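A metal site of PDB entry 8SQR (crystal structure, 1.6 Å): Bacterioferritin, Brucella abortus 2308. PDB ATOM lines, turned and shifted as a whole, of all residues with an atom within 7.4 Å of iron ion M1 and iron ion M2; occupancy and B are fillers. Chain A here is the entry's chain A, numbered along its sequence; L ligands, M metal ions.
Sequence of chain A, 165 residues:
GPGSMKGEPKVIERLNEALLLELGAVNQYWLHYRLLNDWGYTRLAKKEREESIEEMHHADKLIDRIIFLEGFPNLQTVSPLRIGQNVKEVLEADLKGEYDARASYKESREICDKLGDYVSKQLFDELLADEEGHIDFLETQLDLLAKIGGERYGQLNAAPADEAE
OH of Tyr 105 lies close to OE2 of Glu 22 (2.6 Å).
ND1 of His 58 sits close to OE1 of Glu 55 (3.1 Å).
The side-chain carboxylate of Glu 98 sits close to the side-chain hydroxyl of Tyr 29 (2.7 Å).
The side-chain carboxylate (OD2) of Asp 130 sits at hydrogen-bond distance from a ring nitrogen (NE2) of His 58 (3.1 Å).
His 58 touches iron ion M1 (ND1 to FE, 3.0 Å).
Of the 26 residues printed, 4 come within 4 Å of iron ion M1.
OE1 of Glu 98 is bound to iron ion M2 (2.2 Å).
OE1 of Glu 131 is bound to iron ion M2, 2.3 Å away.
OE2 of Glu 55 is bound to iron ion M2.
An oxygen (O1) of the ligand binds iron ion M2 (2.4 Å).
Iron ion M2 is bound by OE2 of Glu 98, at 2.4 Å.
A ring nitrogen (ND1) of His 134 binds iron ion M2, 2.4 Å away.
The side-chain carboxylate (OE2) of Glu 22 is bound to iron ion M1 (2.3 Å).
Iron ion M1 is bound by OE1 of Glu 55 (2.3 Å).
An oxygen (O2) of the ligand binds iron ion M1 (2.3 Å).
OE1 of Glu 22 is bound to iron ion M1 (2.4 Å).
Iron ion M1 is bound by OE2 of Glu 131 (2.4 Å).
Iron ion M1 has five donor atoms within binding distance.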
ATOM      1  N   ALA A  18     -14.818 -25.095 -31.361  1.00  0.00           N
ATOM      2  CA  ALA A  18     -14.059 -24.336 -30.382  1.00  0.00           C
ATOM      3  C   ALA A  18     -14.976 -23.745 -29.318  1.00  0.00           C
ATOM      4  O   ALA A  18     -14.636 -23.738 -28.129  1.00  0.00           O
ATOM      5  CB  ALA A  18     -13.271 -23.236 -31.086  1.00  0.00           C
ATOM      6  N   LEU A  21     -15.738 -26.261 -26.691  1.00  0.00           N
ATOM      7  CA  LEU A  21     -14.606 -26.492 -25.792  1.00  0.00           C
ATOM      8  C   LEU A  21     -14.421 -25.327 -24.841  1.00  0.00           C
ATOM      9  O   LEU A  21     -14.147 -25.516 -23.642  1.00  0.00           O
ATOM     10  CB  LEU A  21     -13.329 -26.732 -26.587  1.00  0.00           C
ATOM     11  CG  LEU A  21     -13.314 -27.952 -27.476  1.00  0.00           C
ATOM     12  CD1 LEU A  21     -12.015 -28.023 -28.267  1.00  0.00           C
ATOM     13  CD2 LEU A  21     -13.536 -29.209 -26.661  1.00  0.00           C
ATOM     14  N   GLU A  22     -14.568 -24.100 -25.330  1.00  0.00           N
ATOM     15  CA  GLU A  22     -14.387 -22.941 -24.464  1.00  0.00           C
ATOM     16  C   GLU A  22     -15.468 -22.863 -23.393  1.00  0.00           C
ATOM     17  O   GLU A  22     -15.166 -22.596 -22.215  1.00  0.00           O
ATOM     18  CB  GLU A  22     -14.373 -21.655 -25.307  1.00  0.00           C
ATOM     19  CG  GLU A  22     -13.187 -21.586 -26.243  1.00  0.00           C
ATOM     20  CD  GLU A  22     -11.940 -21.448 -25.474  1.00  0.00           C
ATOM     21  OE1 GLU A  22     -12.039 -21.018 -24.299  1.00  0.00           O
ATOM     22  OE2 GLU A  22     -10.893 -21.796 -26.004  1.00  0.00           O
ATOM     23  N   LEU A  23     -16.738 -23.060 -23.777  1.00  0.00           N
ATOM     24  CA  LEU A  23     -17.799 -23.085 -22.781  1.00  0.00           C
ATOM     25  C   LEU A  23     -17.606 -24.225 -21.792  1.00  0.00           C
ATOM     26  O   LEU A  23     -17.922 -24.080 -20.607  1.00  0.00           O
ATOM     27  CB  LEU A  23     -19.152 -23.208 -23.471  1.00  0.00           C
ATOM     28  CG  LEU A  23     -19.516 -21.982 -24.319  1.00  0.00           C
ATOM     29  CD1 LEU A  23     -20.738 -22.290 -25.144  1.00  0.00           C
ATOM     30  CD2 LEU A  23     -19.744 -20.780 -23.434  1.00  0.00           C
ATOM     31  N   ALA A  25     -14.741 -25.288 -20.737  1.00  0.00           N
ATOM     32  CA  ALA A  25     -13.692 -24.823 -19.842  1.00  0.00           C
ATOM     33  C   ALA A  25     -14.206 -23.737 -18.904  1.00  0.00           C
ATOM     34  O   ALA A  25     -13.821 -23.703 -17.729  1.00  0.00           O
ATOM     35  CB  ALA A  25     -12.510 -24.294 -20.625  1.00  0.00           C
ATOM     36  N   VAL A  26     -15.067 -22.835 -19.389  1.00  0.00           N
ATOM     37  CA  VAL A  26     -15.680 -21.894 -18.472  1.00  0.00           C
ATOM     38  C   VAL A  26     -16.318 -22.648 -17.312  1.00  0.00           C
ATOM     39  O   VAL A  26     -16.106 -22.318 -16.149  1.00  0.00           O
ATOM     40  CB  VAL A  26     -16.742 -21.028 -19.182  1.00  0.00           C
ATOM     41  CG1 VAL A  26     -17.539 -20.260 -18.118  1.00  0.00           C
ATOM     42  CG2 VAL A  26     -16.114 -20.068 -20.164  1.00  0.00           C
ATOM     43  N   TYR A  29     -13.633 -24.600 -15.043  1.00  0.00           N
ATOM     44  CA  TYR A  29     -12.859 -23.715 -14.174  1.00  0.00           C
ATOM     45  C   TYR A  29     -13.750 -23.104 -13.086  1.00  0.00           C
ATOM     46  O   TYR A  29     -13.305 -22.920 -11.940  1.00  0.00           O
ATOM     47  CB  TYR A  29     -12.156 -22.632 -15.009  1.00  0.00           C
ATOM     48  CG  TYR A  29     -10.872 -23.075 -15.673  1.00  0.00           C
ATOM     49  CD1 TYR A  29      -9.783 -23.443 -14.920  1.00  0.00           C
ATOM     50  CD2 TYR A  29     -10.746 -23.061 -17.047  1.00  0.00           C
ATOM     51  CE1 TYR A  29      -8.576 -23.839 -15.533  1.00  0.00           C
ATOM     52  CE2 TYR A  29      -9.554 -23.465 -17.687  1.00  0.00           C
ATOM     53  CZ  TYR A  29      -8.475 -23.850 -16.901  1.00  0.00           C
ATOM     54  OH  TYR A  29      -7.283 -24.236 -17.501  1.00  0.00           O
ATOM     55  N   GLU A  51      -9.130 -17.661 -14.538  1.00  0.00           N
ATOM     56  CA  GLU A  51      -9.004 -18.400 -15.794  1.00  0.00           C
ATOM     57  C   GLU A  51     -10.366 -18.658 -16.422  1.00  0.00           C
ATOM     58  O   GLU A  51     -10.500 -18.625 -17.654  1.00  0.00           O
ATOM     59  CB  GLU A  51      -8.301 -19.739 -15.568  1.00  0.00           C
ATOM     60  CG  GLU A  51      -6.834 -19.655 -15.098  1.00  0.00           C
ATOM     61  CD  GLU A  51      -5.866 -19.255 -16.211  1.00  0.00           C
ATOM     62  OE1 GLU A  51      -6.271 -18.537 -17.144  1.00  0.00           O
ATOM     63  OE2 GLU A  51      -4.683 -19.678 -16.142  1.00  0.00           O
ATOM     64  N   GLU A  54     -11.345 -15.580 -18.235  1.00  0.00           N
ATOM     65  CA  GLU A  54     -10.634 -15.463 -19.510  1.00  0.00           C
ATOM     66  C   GLU A  54     -11.256 -16.346 -20.578  1.00  0.00           C
ATOM     67  O   GLU A  54     -11.359 -15.922 -21.733  1.00  0.00           O
ATOM     68  CB  GLU A  54      -9.158 -15.831 -19.323  1.00  0.00           C
ATOM     69  CG  GLU A  54      -8.426 -14.753 -18.604  1.00  0.00           C
ATOM     70  CD  GLU A  54      -6.951 -14.902 -18.746  1.00  0.00           C
ATOM     71  OE1 GLU A  54      -6.485 -15.446 -19.775  1.00  0.00           O
ATOM     72  OE2 GLU A  54      -6.267 -14.477 -17.818  1.00  0.00           O
ATOM     73  N   GLU A  55     -11.657 -17.561 -20.210  1.00  0.00           N
ATOM     74  CA  GLU A  55     -12.292 -18.421 -21.196  1.00  0.00           C
ATOM     75  C   GLU A  55     -13.622 -17.823 -21.631  1.00  0.00           C
ATOM     76  O   GLU A  55     -14.030 -18.012 -22.785  1.00  0.00           O
ATOM     77  CB  GLU A  55     -12.510 -19.853 -20.672  1.00  0.00           C
ATOM     78  CG  GLU A  55     -11.275 -20.580 -20.051  1.00  0.00           C
ATOM     79  CD  GLU A  55     -10.201 -20.924 -21.044  1.00  0.00           C
ATOM     80  OE1 GLU A  55     -10.217 -20.359 -22.134  1.00  0.00           O
ATOM     81  OE2 GLU A  55      -9.327 -21.760 -20.723  1.00  0.00           O
ATOM     82  N   MET A  56     -14.312 -17.106 -20.728  1.00  0.00           N
ATOM     83  CA  MET A  56     -15.554 -16.423 -21.124  1.00  0.00           C
ATOM     84  C   MET A  56     -15.307 -15.422 -22.239  1.00  0.00           C
ATOM     85  O   MET A  56     -16.074 -15.331 -23.195  1.00  0.00           O
ATOM     86  CB  MET A  56     -16.160 -15.707 -19.914  1.00  0.00           C
ATOM     87  CG  MET A  56     -16.656 -16.600 -18.811  1.00  0.00           C
ATOM     88  SD  MET A  56     -17.140 -15.723 -17.289  1.00  0.00           S
ATOM     89  CE  MET A  56     -16.881 -16.979 -16.035  1.00  0.00           C
ATOM     90  N   HIS A  58     -12.893 -15.603 -24.434  1.00  0.00           N
ATOM     91  CA  HIS A  58     -12.653 -16.405 -25.638  1.00  0.00           C
ATOM     92  C   HIS A  58     -13.964 -16.843 -26.285  1.00  0.00           C
ATOM     93  O   HIS A  58     -14.147 -16.735 -27.508  1.00  0.00           O
ATOM     94  CB  HIS A  58     -11.833 -17.646 -25.334  1.00  0.00           C
ATOM     95  CG  HIS A  58     -10.435 -17.373 -24.889  1.00  0.00           C
ATOM     96  ND1 HIS A  58      -9.617 -18.347 -24.361  1.00  0.00           N
ATOM     97  CD2 HIS A  58      -9.710 -16.228 -24.880  1.00  0.00           C
ATOM     98  CE1 HIS A  58      -8.451 -17.821 -24.050  1.00  0.00           C
ATOM     99  NE2 HIS A  58      -8.482 -16.529 -24.353  1.00  0.00           N
ATOM    100  N   ALA A  59     -14.882 -17.392 -25.477  1.00  0.00           N
ATOM    101  CA  ALA A  59     -16.187 -17.775 -25.998  1.00  0.00           C
ATOM    102  C   ALA A  59     -16.884 -16.599 -26.676  1.00  0.00           C
ATOM    103  O   ALA A  59     -17.471 -16.767 -27.762  1.00  0.00           O
ATOM    104  CB  ALA A  59     -17.054 -18.339 -24.872  1.00  0.00           C
ATOM    105  N   LEU A  62     -15.512 -15.986 -30.114  1.00  0.00           N
ATOM    106  CA  LEU A  62     -15.952 -17.002 -31.070  1.00  0.00           C
ATOM    107  C   LEU A  62     -17.395 -16.752 -31.495  1.00  0.00           C
ATOM    108  O   LEU A  62     -17.732 -16.861 -32.680  1.00  0.00           O
ATOM    109  CB  LEU A  62     -15.781 -18.412 -30.476  1.00  0.00           C
ATOM    110  CG  LEU A  62     -14.350 -18.927 -30.369  1.00  0.00           C
ATOM    111  CD1 LEU A  62     -14.254 -20.083 -29.373  1.00  0.00           C
ATOM    112  CD2 LEU A  62     -13.813 -19.370 -31.714  1.00  0.00           C
ATOM    113  N   ASP A  94      -7.863 -29.816 -15.627  1.00  0.00           N
ATOM    114  CA  ASP A  94      -7.660 -28.595 -16.393  1.00  0.00           C
ATOM    115  C   ASP A  94      -6.680 -28.827 -17.525  1.00  0.00           C
ATOM    116  O   ASP A  94      -6.913 -28.436 -18.677  1.00  0.00           O
ATOM    117  CB  ASP A  94      -7.116 -27.488 -15.493  1.00  0.00           C
ATOM    118  CG  ASP A  94      -8.089 -27.027 -14.411  1.00  0.00           C
ATOM    119  OD1 ASP A  94      -9.302 -27.186 -14.580  1.00  0.00           O
ATOM    120  OD2 ASP A  94      -7.585 -26.484 -13.391  1.00  0.00           O
ATOM    121  N   GLY A  97      -7.962 -30.721 -20.508  1.00  0.00           N
ATOM    122  CA  GLY A  97      -8.800 -29.864 -21.323  1.00  0.00           C
ATOM    123  C   GLY A  97      -7.977 -28.957 -22.223  1.00  0.00           C
ATOM    124  O   GLY A  97      -8.351 -28.717 -23.378  1.00  0.00           O
ATOM    125  N   GLU A  98      -6.862 -28.436 -21.715  1.00  0.00           N
ATOM    126  CA  GLU A  98      -6.055 -27.522 -22.507  1.00  0.00           C
ATOM    127  C   GLU A  98      -5.378 -28.258 -23.666  1.00  0.00           C
ATOM    128  O   GLU A  98      -5.315 -27.746 -24.792  1.00  0.00           O
ATOM    129  CB  GLU A  98      -5.021 -26.815 -21.628  1.00  0.00           C
ATOM    130  CG  GLU A  98      -5.591 -25.949 -20.483  1.00  0.00           C
ATOM    131  CD  GLU A  98      -6.366 -24.734 -20.921  1.00  0.00           C
ATOM    132  OE1 GLU A  98      -6.121 -24.269 -22.029  1.00  0.00           O
ATOM    133  OE2 GLU A  98      -7.246 -24.221 -20.160  1.00  0.00           O
ATOM    134  N   ALA A 101      -7.998 -28.772 -26.343  1.00  0.00           N
ATOM    135  CA  ALA A 101      -8.258 -27.528 -27.084  1.00  0.00           C
ATOM    136  C   ALA A 101      -7.108 -27.209 -28.029  1.00  0.00           C
ATOM    137  O   ALA A 101      -7.330 -26.850 -29.196  1.00  0.00           O
ATOM    138  CB  ALA A 101      -8.485 -26.381 -26.102  1.00  0.00           C
ATOM    139  N   TYR A 105      -7.409 -26.556 -32.018  1.00  0.00           N
ATOM    140  CA  TYR A 105      -7.122 -25.279 -32.667  1.00  0.00           C
ATOM    141  C   TYR A 105      -6.004 -25.395 -33.703  1.00  0.00           C
ATOM    142  O   TYR A 105      -6.028 -24.661 -34.709  1.00  0.00           O
ATOM    143  CB  TYR A 105      -6.787 -24.230 -31.592  1.00  0.00           C
ATOM    144  CG  TYR A 105      -7.895 -24.053 -30.575  1.00  0.00           C
ATOM    145  CD1 TYR A 105      -9.191 -24.484 -30.856  1.00  0.00           C
ATOM    146  CD2 TYR A 105      -7.647 -23.482 -29.314  1.00  0.00           C
ATOM    147  CE1 TYR A 105     -10.210 -24.359 -29.933  1.00  0.00           C
ATOM    148  CE2 TYR A 105      -8.698 -23.330 -28.381  1.00  0.00           C
ATOM    149  CZ  TYR A 105      -9.966 -23.779 -28.732  1.00  0.00           C
ATOM    150  OH  TYR A 105     -11.020 -23.677 -27.839  1.00  0.00           O
ATOM    151  N   LEU A 127      -5.891 -18.134 -30.060  1.00  0.00           N
ATOM    152  CA  LEU A 127      -6.335 -19.124 -29.085  1.00  0.00           C
ATOM    153  C   LEU A 127      -5.250 -20.158 -28.813  1.00  0.00           C
ATOM    154  O   LEU A 127      -5.016 -20.548 -27.662  1.00  0.00           O
ATOM    155  CB  LEU A 127      -7.613 -19.815 -29.564  1.00  0.00           C
ATOM    156  CG  LEU A 127      -8.851 -18.951 -29.648  1.00  0.00           C
ATOM    157  CD1 LEU A 127      -9.988 -19.762 -30.253  1.00  0.00           C
ATOM    158  CD2 LEU A 127      -9.247 -18.397 -28.285  1.00  0.00           C
ATOM    159  N   ASP A 130      -2.651 -18.753 -26.559  1.00  0.00           N
ATOM    160  CA  ASP A 130      -3.198 -18.661 -25.206  1.00  0.00           C
ATOM    161  C   ASP A 130      -3.195 -20.024 -24.522  1.00  0.00           C
ATOM    162  O   ASP A 130      -2.799 -20.146 -23.361  1.00  0.00           O
ATOM    163  CB  ASP A 130      -4.628 -18.092 -25.244  1.00  0.00           C
ATOM    164  CG  ASP A 130      -4.679 -16.611 -25.568  1.00  0.00           C
ATOM    165  OD1 ASP A 130      -3.616 -15.953 -25.623  1.00  0.00           O
ATOM    166  OD2 ASP A 130      -5.800 -16.099 -25.771  1.00  0.00           O
ATOM    167  N   GLU A 131      -3.644 -21.071 -25.241  1.00  0.00           N
ATOM    168  CA  GLU A 131      -3.689 -22.396 -24.642  1.00  0.00           C
ATOM    169  C   GLU A 131      -2.287 -22.888 -24.264  1.00  0.00           C
ATOM    170  O   GLU A 131      -2.108 -23.547 -23.227  1.00  0.00           O
ATOM    171  CB  GLU A 131      -4.364 -23.418 -25.567  1.00  0.00           C
ATOM    172  CG  GLU A 131      -5.756 -23.088 -26.109  1.00  0.00           C
ATOM    173  CD  GLU A 131      -6.763 -22.770 -25.042  1.00  0.00           C
ATOM    174  OE1 GLU A 131      -6.396 -22.928 -23.881  1.00  0.00           O
ATOM    175  OE2 GLU A 131      -7.891 -22.341 -25.359  1.00  0.00           O
ATOM    176  N   GLU A 132      -1.282 -22.653 -25.125  1.00  0.00           N
ATOM    177  CA  GLU A 132       0.070 -23.060 -24.740  1.00  0.00           C
ATOM    178  C   GLU A 132       0.536 -22.298 -23.500  1.00  0.00           C
ATOM    179  O   GLU A 132       1.233 -22.866 -22.655  1.00  0.00           O
ATOM    180  CB  GLU A 132       1.039 -22.911 -25.928  1.00  0.00           C
ATOM    181  CG  GLU A 132       0.743 -23.975 -27.009  1.00  0.00           C
ATOM    182  CD  GLU A 132       1.832 -24.222 -28.056  1.00  0.00           C
ATOM    183  OE1 GLU A 132       2.945 -23.671 -27.956  1.00  0.00           O
ATOM    184  OE2 GLU A 132       1.564 -24.991 -29.020  1.00  0.00           O
ATOM    185  N   HIS A 134      -1.500 -21.394 -20.998  1.00  0.00           N
ATOM    186  CA  HIS A 134      -2.172 -22.106 -19.909  1.00  0.00           C
ATOM    187  C   HIS A 134      -1.495 -23.438 -19.626  1.00  0.00           C
ATOM    188  O   HIS A 134      -1.385 -23.860 -18.465  1.00  0.00           O
ATOM    189  CB  HIS A 134      -3.657 -22.336 -20.258  1.00  0.00           C
ATOM    190  CG  HIS A 134      -4.453 -21.087 -20.485  1.00  0.00           C
ATOM    191  ND1 HIS A 134      -5.683 -21.102 -21.105  1.00  0.00           N
ATOM    192  CD2 HIS A 134      -4.216 -19.791 -20.179  1.00  0.00           C
ATOM    193  CE1 HIS A 134      -6.164 -19.872 -21.181  1.00  0.00           C
ATOM    194  NE2 HIS A 134      -5.290 -19.056 -20.627  1.00  0.00           N
ATOM    195  N   ILE A 135      -1.086 -24.162 -20.678  1.00  0.00           N
ATOM    196  CA  ILE A 135      -0.370 -25.423 -20.496  1.00  0.00           C
ATOM    197  C   ILE A 135       0.931 -25.183 -19.733  1.00  0.00           C
ATOM    198  O   ILE A 135       1.260 -25.913 -18.788  1.00  0.00           O
ATOM    199  CB  ILE A 135      -0.112 -26.096 -21.861  1.00  0.00           C
ATOM    200  CG1 ILE A 135      -1.453 -26.591 -22.453  1.00  0.00           C
ATOM    201  CG2 ILE A 135       0.855 -27.247 -21.722  1.00  0.00           C
ATOM    202  CD1 ILE A 135      -1.366 -26.853 -23.940  1.00  0.00           C
ATOM    203  N   LEU A 138       0.031 -24.604 -16.056  1.00  0.00           N
ATOM    204  CA  LEU A 138      -0.442 -25.784 -15.361  1.00  0.00           C
ATOM    205  C   LEU A 138       0.659 -26.823 -15.196  1.00  0.00           C
ATOM    206  O   LEU A 138       0.730 -27.481 -14.163  1.00  0.00           O
ATOM    207  CB  LEU A 138      -1.642 -26.390 -16.081  1.00  0.00           C
ATOM    208  CG  LEU A 138      -2.949 -25.638 -15.970  1.00  0.00           C
ATOM    209  CD1 LEU A 138      -3.883 -26.166 -17.044  1.00  0.00           C
ATOM    210  CD2 LEU A 138      -3.563 -25.822 -14.592  1.00  0.00           C
HETATM  211  C1  LIG L   1      -9.703 -24.504 -23.152  1.00  0.00           C
HETATM  212  O1  LIG L   1      -8.938 -24.406 -22.173  1.00  0.00           O
HETATM  213  O2  LIG L   1      -9.923 -23.611 -23.987  1.00  0.00           O
HETATM  214  C2  LIG L   1     -10.427 -25.867 -23.279  1.00  0.00           C
HETATM  215 FE    FE M   1      -9.708 -21.309 -24.147  1.00  0.00          FE
HETATM  216 FE    FE M   2      -7.464 -22.581 -21.896  1.00  0.00          FE
